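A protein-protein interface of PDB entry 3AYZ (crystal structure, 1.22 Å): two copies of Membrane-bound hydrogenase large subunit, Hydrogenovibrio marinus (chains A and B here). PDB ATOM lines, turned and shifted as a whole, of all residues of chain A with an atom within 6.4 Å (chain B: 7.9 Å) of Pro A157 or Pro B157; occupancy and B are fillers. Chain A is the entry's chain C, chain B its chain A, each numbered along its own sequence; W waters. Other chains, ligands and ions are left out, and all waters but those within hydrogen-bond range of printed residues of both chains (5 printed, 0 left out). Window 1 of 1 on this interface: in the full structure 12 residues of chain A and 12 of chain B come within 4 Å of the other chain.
The backbone carbonyl oxygen (O) of Pro B157 sits at hydrogen-bond distance from the side-chain hydroxyl (OG) of Ser A160, at 2.9 Å. N of Ser B159 is in hydrogen-bond range of O of Pro A157, 3.2 Å away. The backbone NH of Ser A159 is in hydrogen-bond range of the backbone carbonyl oxygen of Pro B157, 3.1 Å away. OG of Ser B160 sits at hydrogen-bond distance from O of Pro A157 (3.0 Å). OG of Ser B159 sits at hydrogen-bond distance from OG of Ser A160. OG of Ser B160 sits at hydrogen-bond distance from O of His A156 (2.6 Å). The side-chain hydroxyl (OG) of Ser B160 lies within hydrogen-bond range of the side-chain hydroxyl (OG) of Ser A159 (2.6 Å). The side-chain hydroxyl (OG) of Ser A160 lies within hydrogen-bond range of the backbone carbonyl oxygen (O) of His B156, 2.6 Å away. The side-chain sulfur (SD) of Met B158 lies close to the side-chain sulfur (SD) of Met A158, 3.4 Å away. OD2 of Asp B166 sits at hydrogen-bond distance from ND1 of His A155 (2.7 Å). O of Pro A157 lies close to O of Pro B157 (3.2 Å).
A ring nitrogen (NE2) of His B156 sits at hydrogen-bond distance from the side-chain carboxylate (OE1) of Glu B209, 2.8 Å away. The side-chain hydroxyl of Ser B146 lies within hydrogen-bond range of the backbone carbonyl oxygen of Ser B159 (2.7 Å). The side-chain hydroxyl (OH) of Tyr B163 lies within hydrogen-bond range of the side-chain carboxylate (OE2) of Glu B209, at 2.6 Å.
Among the printed residues, pairs that only touch across the chains: Pro A154 with Gly B162, Pro A157 with Met B158, Met A158 with Pro B157, Tyr A163 with Pro B157, Pro A157 with Tyr B163, Met A158 with Ser B160, Ser A159 with Ser B159 and Ser A160 with Met B158.
Of the printed residues of chain B, Pro A157 touches Pro B157, Met B158, Ser B159, Ser B160 and Tyr B163. Printed residues of chain A within 4 Å of Pro B157: Pro A157, Met A158, Ser A159, Ser A160 and Tyr A163. Of the printed residues of chain A, His B156 touches Ser A160 (2.6 Å). Printed residues of chain B within 4 Å of Met A158: Pro B157, Met B158 and Ser B160. The nearest printed residue of chain B that does not touch Pro A157 is Gly B162 (6.5 Å).
Of the 11 printed residues of chain A, 8 touch a printed residue of chain B. Hydrophobic or aromatic side chains of chain A that line the printed part of chain B: His A155, Pro A157, Met A158 and Tyr A163. Along chain A the printed residues that touch a printed residue of chain B span positions 154 to 163. Printed residues of chain B that touch a printed residue of chain A: His B156, Pro B157, Met B158, Ser B159, Ser B160, Gly B162, Tyr B163 and Asp B166. Hydrophobic or aromatic side chains of chain B within 4 Å of the printed part of chain A: Pro B157, Met B158 and Tyr B163. Among the printed residues, no Asp or Glu carboxylate lies within 4 Å of a Lys or Arg side-chain nitrogen of the other chain.
Pro A157 touches Ser B159, and with the chains exchanged Ser A159 touches Pro B157. Pro A157 touches Tyr B163, and with the chains exchanged Tyr A163 touches Pro B157. Met B158 touches its own counterpart, Met A158. Met A158 touches Ser B160, and with the chains exchanged Ser A160 touches Met B158.
Water W5 lies within hydrogen-bond range of O of Ser A153 (2.7 Å), O of His A156 (2.8 Å), OG of Ser B160 (3.3 Å) and NE2 of Gln A149 (3.4 Å). Water W3 bridges O of Pro A154 (2.7 Å) and N of Gly B162 (2.9 Å). Water W1 bridges OD2 of Asp B166 (2.7 Å) and O of His A155 (2.7 Å). Water W4 lies within hydrogen-bond range of the backbone carbonyl oxygen (O) of Ser B153 (2.8 Å), the backbone carbonyl oxygen (O) of His B156 (2.8 Å), the side-chain amide nitrogen (NE2) of Gln B149 (3.2 Å) and the side-chain hydroxyl (OG) of Ser A160 (3.4 Å). Water W2 lies within hydrogen-bond range of the side-chain hydroxyl of Ser B159 and the side-chain hydroxyl of Ser A159.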
ATOM      1  N   GLN A 149      -9.100 -16.045  24.957  1.00  0.00           N
ATOM      2  CA  GLN A 149      -8.818 -15.301  26.164  1.00  0.00           C
ATOM      3  C   GLN A 149      -9.807 -15.646  27.241  1.00  0.00           C
ATOM      4  O   GLN A 149      -9.379 -15.829  28.396  1.00  0.00           O
ATOM      5  CB  GLN A 149      -8.830 -13.832  25.856  1.00  0.00           C
ATOM      6  CG  GLN A 149      -8.776 -12.865  27.021  1.00  0.00           C
ATOM      7  CD  GLN A 149      -7.454 -12.877  27.725  1.00  0.00           C
ATOM      8  OE1 GLN A 149      -6.400 -12.762  27.159  1.00  0.00           O
ATOM      9  NE2 GLN A 149      -7.501 -13.094  29.005  1.00  0.00           N
ATOM     10  N   SER A 153      -8.361 -17.314  30.755  1.00  0.00           N
ATOM     11  CA  SER A 153      -8.424 -16.564  31.986  1.00  0.00           C
ATOM     12  C   SER A 153      -9.764 -15.852  32.080  1.00  0.00           C
ATOM     13  O   SER A 153      -9.841 -14.671  31.735  1.00  0.00           O
ATOM     14  CB  SER A 153      -7.271 -15.566  32.101  1.00  0.00           C
ATOM     15  OG  SER A 153      -7.339 -15.065  33.421  1.00  0.00           O
ATOM     16  N   PRO A 154     -10.779 -16.510  32.547  1.00  0.00           N
ATOM     17  CA  PRO A 154     -12.129 -15.894  32.575  1.00  0.00           C
ATOM     18  C   PRO A 154     -12.228 -14.618  33.366  1.00  0.00           C
ATOM     19  O   PRO A 154     -13.065 -13.781  33.062  1.00  0.00           O
ATOM     20  CB  PRO A 154     -12.981 -17.011  33.162  1.00  0.00           C
ATOM     21  CG  PRO A 154     -12.230 -18.223  33.167  1.00  0.00           C
ATOM     22  CD  PRO A 154     -10.780 -17.923  32.991  1.00  0.00           C
ATOM     23  N   HIS A 155     -11.435 -14.423  34.418  1.00  0.00           N
ATOM     24  CA  HIS A 155     -11.554 -13.246  35.204  1.00  0.00           C
ATOM     25  C   HIS A 155     -10.796 -12.037  34.645  1.00  0.00           C
ATOM     26  O   HIS A 155     -11.056 -10.896  35.070  1.00  0.00           O
ATOM     27  CB  HIS A 155     -11.002 -13.491  36.626  1.00  0.00           C
ATOM     28  CG  HIS A 155     -11.854 -14.420  37.434  1.00  0.00           C
ATOM     29  ND1 HIS A 155     -12.942 -14.081  38.138  1.00  0.00           N
ATOM     30  CD2 HIS A 155     -11.651 -15.737  37.608  1.00  0.00           C
ATOM     31  CE1 HIS A 155     -13.411 -15.163  38.736  1.00  0.00           C
ATOM     32  NE2 HIS A 155     -12.641 -16.213  38.415  1.00  0.00           N
ATOM     33  N   HIS A 156      -9.876 -12.234  33.712  1.00  0.00           N
ATOM     34  CA  HIS A 156      -9.147 -11.069  33.239  1.00  0.00           C
ATOM     35  C   HIS A 156     -10.091 -10.175  32.445  1.00  0.00           C
ATOM     36  O   HIS A 156     -10.738 -10.666  31.524  1.00  0.00           O
ATOM     37  CB  HIS A 156      -7.969 -11.473  32.320  1.00  0.00           C
ATOM     38  CG  HIS A 156      -7.076 -10.362  31.961  1.00  0.00           C
ATOM     39  ND1 HIS A 156      -6.656  -9.442  32.868  1.00  0.00           N
ATOM     40  CD2 HIS A 156      -6.428 -10.078  30.808  1.00  0.00           C
ATOM     41  CE1 HIS A 156      -5.808  -8.626  32.284  1.00  0.00           C
ATOM     42  NE2 HIS A 156      -5.641  -8.971  31.032  1.00  0.00           N
ATOM     43  N   PRO A 157     -10.211  -8.905  32.782  1.00  0.00           N
ATOM     44  CA  PRO A 157     -11.216  -8.092  32.081  1.00  0.00           C
ATOM     45  C   PRO A 157     -10.939  -7.797  30.608  1.00  0.00           C
ATOM     46  O   PRO A 157     -11.866  -7.482  29.873  1.00  0.00           O
ATOM     47  CB  PRO A 157     -11.241  -6.747  32.846  1.00  0.00           C
ATOM     48  CG  PRO A 157     -10.810  -7.199  34.203  1.00  0.00           C
ATOM     49  CD  PRO A 157      -9.682  -8.175  33.943  1.00  0.00           C
ATOM     50  N   MET A 158      -9.680  -7.841  30.170  1.00  0.00           N
ATOM     51  CA  MET A 158      -9.213  -7.257  28.920  1.00  0.00           C
ATOM     52  C   MET A 158      -9.381  -8.266  27.783  1.00  0.00           C
ATOM     53  O   MET A 158      -8.417  -8.920  27.366  1.00  0.00           O
ATOM     54  CB  MET A 158      -7.726  -6.839  28.985  1.00  0.00           C
ATOM     55  CG  MET A 158      -7.250  -5.928  30.047  1.00  0.00           C
ATOM     56  SD  MET A 158      -7.882  -4.249  29.878  1.00  0.00           S
ATOM     57  CE  MET A 158      -6.646  -3.702  28.644  1.00  0.00           C
ATOM     58  N   SER A 159     -10.567  -8.466  27.291  1.00  0.00           N
ATOM     59  CA  SER A 159     -10.814  -9.502  26.328  1.00  0.00           C
ATOM     60  C   SER A 159     -11.573  -9.067  25.111  1.00  0.00           C
ATOM     61  O   SER A 159     -11.899  -9.902  24.240  1.00  0.00           O
ATOM     62  CB  SER A 159     -11.585 -10.655  26.980  1.00  0.00           C
ATOM     63  OG  SER A 159     -12.879 -10.277  27.344  1.00  0.00           O
ATOM     64  N   SER A 160     -11.950  -7.786  24.925  1.00  0.00           N
ATOM     65  CA  SER A 160     -12.798  -7.430  23.802  1.00  0.00           C
ATOM     66  C   SER A 160     -12.153  -7.780  22.465  1.00  0.00           C
ATOM     67  O   SER A 160     -10.990  -7.513  22.295  1.00  0.00           O
ATOM     68  CB  SER A 160     -13.055  -5.882  23.740  1.00  0.00           C
ATOM     69  OG  SER A 160     -13.581  -5.547  25.011  1.00  0.00           O
ATOM     70  N   TYR A 163     -10.377  -4.757  21.170  1.00  0.00           N
ATOM     71  CA  TYR A 163      -9.066  -4.582  21.803  1.00  0.00           C
ATOM     72  C   TYR A 163      -8.018  -5.411  21.109  1.00  0.00           C
ATOM     73  O   TYR A 163      -6.958  -4.899  20.716  1.00  0.00           O
ATOM     74  CB  TYR A 163      -9.141  -4.935  23.251  1.00  0.00           C
ATOM     75  CG  TYR A 163      -7.846  -5.004  24.034  1.00  0.00           C
ATOM     76  CD1 TYR A 163      -6.981  -3.926  24.082  1.00  0.00           C
ATOM     77  CD2 TYR A 163      -7.503  -6.138  24.765  1.00  0.00           C
ATOM     78  CE1 TYR A 163      -5.794  -3.943  24.821  1.00  0.00           C
ATOM     79  CE2 TYR A 163      -6.343  -6.183  25.510  1.00  0.00           C
ATOM     80  CZ  TYR A 163      -5.481  -5.105  25.512  1.00  0.00           C
ATOM     81  OH  TYR A 163      -4.333  -5.147  26.266  1.00  0.00           O
ATOM     82  N   ASN A 275      -4.360 -13.594  37.040  1.00  0.00           N
ATOM     83  CA  ASN A 275      -5.223 -13.396  35.863  1.00  0.00           C
ATOM     84  C   ASN A 275      -4.507 -13.375  34.530  1.00  0.00           C
ATOM     85  O   ASN A 275      -5.179 -13.483  33.489  1.00  0.00           O
ATOM     86  CB  ASN A 275      -6.020 -12.076  35.985  1.00  0.00           C
ATOM     87  CG  ASN A 275      -7.121 -12.131  37.025  1.00  0.00           C
ATOM     88  OD1 ASN A 275      -7.419 -13.148  37.618  1.00  0.00           O
ATOM     89  ND2 ASN A 275      -7.739 -10.986  37.240  1.00  0.00           N
ATOM     90  N   SER B 146     -21.720  -8.581  28.695  1.00  0.00           N
ATOM     91  CA  SER B 146     -20.569  -8.536  27.840  1.00  0.00           C
ATOM     92  C   SER B 146     -21.025  -8.253  26.401  1.00  0.00           C
ATOM     93  O   SER B 146     -20.422  -7.431  25.698  1.00  0.00           O
ATOM     94  CB  SER B 146     -19.785  -9.837  27.999  1.00  0.00           C
ATOM     95  OG  SER B 146     -18.729  -9.878  27.003  1.00  0.00           O
ATOM     96  N   GLN B 149     -21.975  -4.622  26.129  1.00  0.00           N
ATOM     97  CA  GLN B 149     -20.781  -3.815  26.216  1.00  0.00           C
ATOM     98  C   GLN B 149     -20.104  -3.753  24.861  1.00  0.00           C
ATOM     99  O   GLN B 149     -19.672  -2.685  24.458  1.00  0.00           O
ATOM    100  CB  GLN B 149     -19.866  -4.409  27.286  1.00  0.00           C
ATOM    101  CG  GLN B 149     -18.470  -3.855  27.348  1.00  0.00           C
ATOM    102  CD  GLN B 149     -18.404  -2.410  27.764  1.00  0.00           C
ATOM    103  OE1 GLN B 149     -19.025  -2.013  28.727  1.00  0.00           O
ATOM    104  NE2 GLN B 149     -17.688  -1.621  27.030  1.00  0.00           N
ATOM    105  N   LYS B 150     -19.932  -4.912  24.230  1.00  0.00           N
ATOM    106  CA  LYS B 150     -19.194  -4.917  22.941  1.00  0.00           C
ATOM    107  C   LYS B 150     -19.927  -4.146  21.893  1.00  0.00           C
ATOM    108  O   LYS B 150     -19.285  -3.577  21.036  1.00  0.00           O
ATOM    109  CB  LYS B 150     -18.944  -6.384  22.550  1.00  0.00           C
ATOM    110  CG  LYS B 150     -17.939  -7.067  23.426  1.00  0.00           C
ATOM    111  CD  LYS B 150     -17.651  -8.522  23.041  1.00  0.00           C
ATOM    112  CE  LYS B 150     -18.860  -9.418  23.187  1.00  0.00           C
ATOM    113  NZ  LYS B 150     -18.521 -10.787  22.675  1.00  0.00           N
ATOM    114  N   SER B 153     -19.612  -0.134  22.955  1.00  0.00           N
ATOM    115  CA  SER B 153     -18.285   0.446  22.792  1.00  0.00           C
ATOM    116  C   SER B 153     -17.301  -0.624  22.355  1.00  0.00           C
ATOM    117  O   SER B 153     -16.638  -1.200  23.220  1.00  0.00           O
ATOM    118  CB  SER B 153     -17.791   1.125  24.055  1.00  0.00           C
ATOM    119  OG  SER B 153     -16.582   1.825  23.739  1.00  0.00           O
ATOM    120  N   PRO B 154     -17.218  -0.967  21.090  1.00  0.00           N
ATOM    121  CA  PRO B 154     -16.402  -2.081  20.636  1.00  0.00           C
ATOM    122  C   PRO B 154     -14.943  -1.942  20.994  1.00  0.00           C
ATOM    123  O   PRO B 154     -14.269  -2.969  21.169  1.00  0.00           O
ATOM    124  CB  PRO B 154     -16.570  -2.056  19.125  1.00  0.00           C
ATOM    125  CG  PRO B 154     -17.778  -1.281  18.828  1.00  0.00           C
ATOM    126  CD  PRO B 154     -18.007  -0.373  19.969  1.00  0.00           C
ATOM    127  N   HIS B 155     -14.357  -0.778  21.095  1.00  0.00           N
ATOM    128  CA  HIS B 155     -12.962  -0.598  21.356  1.00  0.00           C
ATOM    129  C   HIS B 155     -12.602  -0.704  22.830  1.00  0.00           C
ATOM    130  O   HIS B 155     -11.445  -0.894  23.159  1.00  0.00           O
ATOM    131  CB  HIS B 155     -12.416   0.743  20.851  1.00  0.00           C
ATOM    132  CG  HIS B 155     -12.443   0.876  19.380  1.00  0.00           C
ATOM    133  ND1 HIS B 155     -11.433   0.420  18.604  1.00  0.00           N
ATOM    134  CD2 HIS B 155     -13.364   1.401  18.539  1.00  0.00           C
ATOM    135  CE1 HIS B 155     -11.701   0.637  17.340  1.00  0.00           C
ATOM    136  NE2 HIS B 155     -12.867   1.257  17.255  1.00  0.00           N
ATOM    137  N   HIS B 156     -13.566  -0.552  23.748  1.00  0.00           N
ATOM    138  CA  HIS B 156     -13.202  -0.594  25.172  1.00  0.00           C
ATOM    139  C   HIS B 156     -12.738  -1.994  25.535  1.00  0.00           C
ATOM    140  O   HIS B 156     -13.476  -2.938  25.235  1.00  0.00           O
ATOM    141  CB  HIS B 156     -14.376  -0.185  26.054  1.00  0.00           C
ATOM    142  CG  HIS B 156     -13.946   0.019  27.472  1.00  0.00           C
ATOM    143  ND1 HIS B 156     -12.849   0.720  27.883  1.00  0.00           N
ATOM    144  CD2 HIS B 156     -14.583  -0.318  28.634  1.00  0.00           C
ATOM    145  CE1 HIS B 156     -12.835   0.784  29.189  1.00  0.00           C
ATOM    146  NE2 HIS B 156     -13.884   0.150  29.677  1.00  0.00           N
ATOM    147  N   PRO B 157     -11.554  -2.176  26.074  1.00  0.00           N
ATOM    148  CA  PRO B 157     -11.119  -3.571  26.343  1.00  0.00           C
ATOM    149  C   PRO B 157     -11.859  -4.372  27.386  1.00  0.00           C
ATOM    150  O   PRO B 157     -11.846  -5.602  27.311  1.00  0.00           O
ATOM    151  CB  PRO B 157      -9.657  -3.374  26.785  1.00  0.00           C
ATOM    152  CG  PRO B 157      -9.234  -2.112  26.092  1.00  0.00           C
ATOM    153  CD  PRO B 157     -10.449  -1.226  26.302  1.00  0.00           C
ATOM    154  N   MET B 158     -12.489  -3.676  28.319  1.00  0.00           N
ATOM    155  CA  MET B 158     -12.997  -4.223  29.583  1.00  0.00           C
ATOM    156  C   MET B 158     -14.390  -4.844  29.430  1.00  0.00           C
ATOM    157  O   MET B 158     -15.379  -4.294  29.858  1.00  0.00           O
ATOM    158  CB  MET B 158     -13.013  -3.120  30.650  1.00  0.00           C
ATOM    159  CG  MET B 158     -11.715  -2.328  30.861  1.00  0.00           C
ATOM    160  SD  MET B 158     -10.526  -3.326  31.769  1.00  0.00           S
ATOM    161  CE  MET B 158     -11.209  -3.163  33.430  1.00  0.00           C
ATOM    162  N   SER B 159     -14.495  -6.001  28.745  1.00  0.00           N
ATOM    163  CA  SER B 159     -15.772  -6.560  28.435  1.00  0.00           C
ATOM    164  C   SER B 159     -15.989  -7.982  28.891  1.00  0.00           C
ATOM    165  O   SER B 159     -17.034  -8.546  28.617  1.00  0.00           O
ATOM    166  CB  SER B 159     -16.057  -6.442  26.932  1.00  0.00           C
ATOM    167  OG  SER B 159     -15.155  -7.265  26.202  1.00  0.00           O
ATOM    168  N   SER B 160     -15.021  -8.639  29.550  1.00  0.00           N
ATOM    169  CA  SER B 160     -15.151 -10.040  29.869  1.00  0.00           C
ATOM    170  C   SER B 160     -16.404 -10.334  30.683  1.00  0.00           C
ATOM    171  O   SER B 160     -16.680  -9.643  31.628  1.00  0.00           O
ATOM    172  CB  SER B 160     -13.947 -10.505  30.691  1.00  0.00           C
ATOM    173  OG  SER B 160     -12.748 -10.299  29.976  1.00  0.00           O
ATOM    174  N   PRO B 161     -17.112 -11.406  30.333  1.00  0.00           N
ATOM    175  CA  PRO B 161     -18.246 -11.829  31.196  1.00  0.00           C
ATOM    176  C   PRO B 161     -17.823 -12.023  32.653  1.00  0.00           C
ATOM    177  O   PRO B 161     -18.548 -11.651  33.573  1.00  0.00           O
ATOM    178  CB  PRO B 161     -18.709 -13.131  30.569  1.00  0.00           C
ATOM    179  CG  PRO B 161     -18.250 -13.100  29.151  1.00  0.00           C
ATOM    180  CD  PRO B 161     -17.017 -12.270  29.125  1.00  0.00           C
ATOM    181  N   GLY B 162     -16.657 -12.619  32.824  1.00  0.00           N
ATOM    182  CA  GLY B 162     -16.170 -12.810  34.196  1.00  0.00           C
ATOM    183  C   GLY B 162     -15.872 -11.552  34.981  1.00  0.00           C
ATOM    184  O   GLY B 162     -16.038 -11.523  36.196  1.00  0.00           O
ATOM    185  N   TYR B 163     -15.481 -10.498  34.272  1.00  0.00           N
ATOM    186  CA  TYR B 163     -15.326  -9.195  34.876  1.00  0.00           C
ATOM    187  C   TYR B 163     -16.663  -8.620  35.327  1.00  0.00           C
ATOM    188  O   TYR B 163     -16.785  -8.241  36.487  1.00  0.00           O
ATOM    189  CB  TYR B 163     -14.692  -8.253  33.893  1.00  0.00           C
ATOM    190  CG  TYR B 163     -14.625  -6.802  34.238  1.00  0.00           C
ATOM    191  CD1 TYR B 163     -14.077  -6.334  35.403  1.00  0.00           C
ATOM    192  CD2 TYR B 163     -15.105  -5.830  33.353  1.00  0.00           C
ATOM    193  CE1 TYR B 163     -13.994  -4.993  35.761  1.00  0.00           C
ATOM    194  CE2 TYR B 163     -15.044  -4.469  33.648  1.00  0.00           C
ATOM    195  CZ  TYR B 163     -14.476  -4.032  34.846  1.00  0.00           C
ATOM    196  OH  TYR B 163     -14.373  -2.721  35.195  1.00  0.00           O
ATOM    197  N   PHE B 164     -17.656  -8.660  34.445  1.00  0.00           N
ATOM    198  CA  PHE B 164     -18.973  -8.214  34.899  1.00  0.00           C
ATOM    199  C   PHE B 164     -19.509  -9.068  36.029  1.00  0.00           C
ATOM    200  O   PHE B 164     -20.178  -8.544  36.943  1.00  0.00           O
ATOM    201  CB  PHE B 164     -19.915  -8.196  33.669  1.00  0.00           C
ATOM    202  CG  PHE B 164     -19.616  -7.062  32.703  1.00  0.00           C
ATOM    203  CD1 PHE B 164     -19.678  -5.725  33.136  1.00  0.00           C
ATOM    204  CD2 PHE B 164     -19.266  -7.322  31.397  1.00  0.00           C
ATOM    205  CE1 PHE B 164     -19.410  -4.691  32.252  1.00  0.00           C
ATOM    206  CE2 PHE B 164     -18.975  -6.316  30.501  1.00  0.00           C
ATOM    207  CZ  PHE B 164     -19.040  -4.953  30.936  1.00  0.00           C
ATOM    208  N   ASP B 166     -17.715 -10.547  38.321  1.00  0.00           N
ATOM    209  CA  ASP B 166     -16.970 -10.158  39.516  1.00  0.00           C
ATOM    210  C   ASP B 166     -17.543  -8.855  40.062  1.00  0.00           C
ATOM    211  O   ASP B 166     -17.624  -8.673  41.287  1.00  0.00           O
ATOM    212  CB  ASP B 166     -15.503 -10.116  39.177  1.00  0.00           C
ATOM    213  CG  ASP B 166     -14.849 -11.447  39.045  1.00  0.00           C
ATOM    214  OD1 ASP B 166     -15.466 -12.456  39.507  1.00  0.00           O
ATOM    215  OD2 ASP B 166     -13.728 -11.490  38.495  1.00  0.00           O
ATOM    216  N   ILE B 167     -17.850  -7.879  39.228  1.00  0.00           N
ATOM    217  CA  ILE B 167     -18.489  -6.640  39.693  1.00  0.00           C
ATOM    218  C   ILE B 167     -19.808  -6.932  40.356  1.00  0.00           C
ATOM    219  O   ILE B 167     -20.091  -6.454  41.456  1.00  0.00           O
ATOM    220  CB  ILE B 167     -18.637  -5.628  38.522  1.00  0.00           C
ATOM    221  CG1 ILE B 167     -17.271  -5.210  37.935  1.00  0.00           C
ATOM    222  CG2 ILE B 167     -19.470  -4.430  38.970  1.00  0.00           C
ATOM    223  CD1 ILE B 167     -16.359  -4.418  38.856  1.00  0.00           C
ATOM    224  N   GLU B 209     -15.322   2.323  37.121  1.00  0.00           N
ATOM    225  CA  GLU B 209     -14.177   2.645  36.281  1.00  0.00           C
ATOM    226  C   GLU B 209     -13.946   4.149  36.227  1.00  0.00           C
ATOM    227  O   GLU B 209     -12.809   4.622  36.244  1.00  0.00           O
ATOM    228  CB  GLU B 209     -14.377   2.163  34.827  1.00  0.00           C
ATOM    229  CG  GLU B 209     -14.317   0.615  34.726  1.00  0.00           C
ATOM    230  CD  GLU B 209     -14.448   0.065  33.364  1.00  0.00           C
ATOM    231  OE1 GLU B 209     -14.157   0.787  32.361  1.00  0.00           O
ATOM    232  OE2 GLU B 209     -14.893  -1.098  33.238  1.00  0.00           O
ATOM    233  N   THR B 271      -8.995   8.822  25.545  1.00  0.00           N
ATOM    234  CA  THR B 271      -9.435   7.451  25.442  1.00  0.00           C
ATOM    235  C   THR B 271     -10.650   7.187  26.289  1.00  0.00           C
ATOM    236  O   THR B 271     -11.572   6.481  25.836  1.00  0.00           O
ATOM    237  CB  THR B 271      -8.253   6.510  25.797  1.00  0.00           C
ATOM    238  OG1 THR B 271      -7.239   6.722  24.815  1.00  0.00           O
ATOM    239  CG2 THR B 271      -8.721   5.058  25.761  1.00  0.00           C
ATOM    240  N   ASN B 275     -14.080   5.916  24.606  1.00  0.00           N
ATOM    241  CA  ASN B 275     -14.367   4.518  24.815  1.00  0.00           C
ATOM    242  C   ASN B 275     -15.371   4.212  25.908  1.00  0.00           C
ATOM    243  O   ASN B 275     -15.919   3.094  25.928  1.00  0.00           O
ATOM    244  CB  ASN B 275     -13.086   3.687  25.090  1.00  0.00           C
ATOM    245  CG  ASN B 275     -12.210   3.554  23.859  1.00  0.00           C
ATOM    246  OD1 ASN B 275     -12.566   3.938  22.756  1.00  0.00           O
ATOM    247  ND2 ASN B 275     -11.077   2.936  24.079  1.00  0.00           N
ATOM    248  N   VAL B 276     -15.548   5.110  26.856  1.00  0.00           N
ATOM    249  CA  VAL B 276     -16.431   4.831  27.980  1.00  0.00           C
ATOM    250  C   VAL B 276     -17.584   5.857  28.041  1.00  0.00           C
ATOM    251  O   VAL B 276     -18.742   5.489  27.914  1.00  0.00           O
ATOM    252  CB  VAL B 276     -15.657   4.709  29.311  1.00  0.00           C
ATOM    253  CG1 VAL B 276     -16.621   4.287  30.421  1.00  0.00           C
ATOM    254  CG2 VAL B 276     -14.509   3.714  29.179  1.00  0.00           C
HETATM  255  O   HOH W   1     -12.545  -9.594  36.945  1.00  0.00           O
HETATM  256  O   HOH W   2     -15.308 -10.111  25.793  1.00  0.00           O
HETATM  257  O   HOH W   3     -14.832 -14.033  31.032  1.00  0.00           O
HETATM  258  O   HOH W   4     -16.220  -3.427  24.792  1.00  0.00           O
HETATM  259  O   HOH W   5     -10.748 -12.943  29.874  1.00  0.00           O
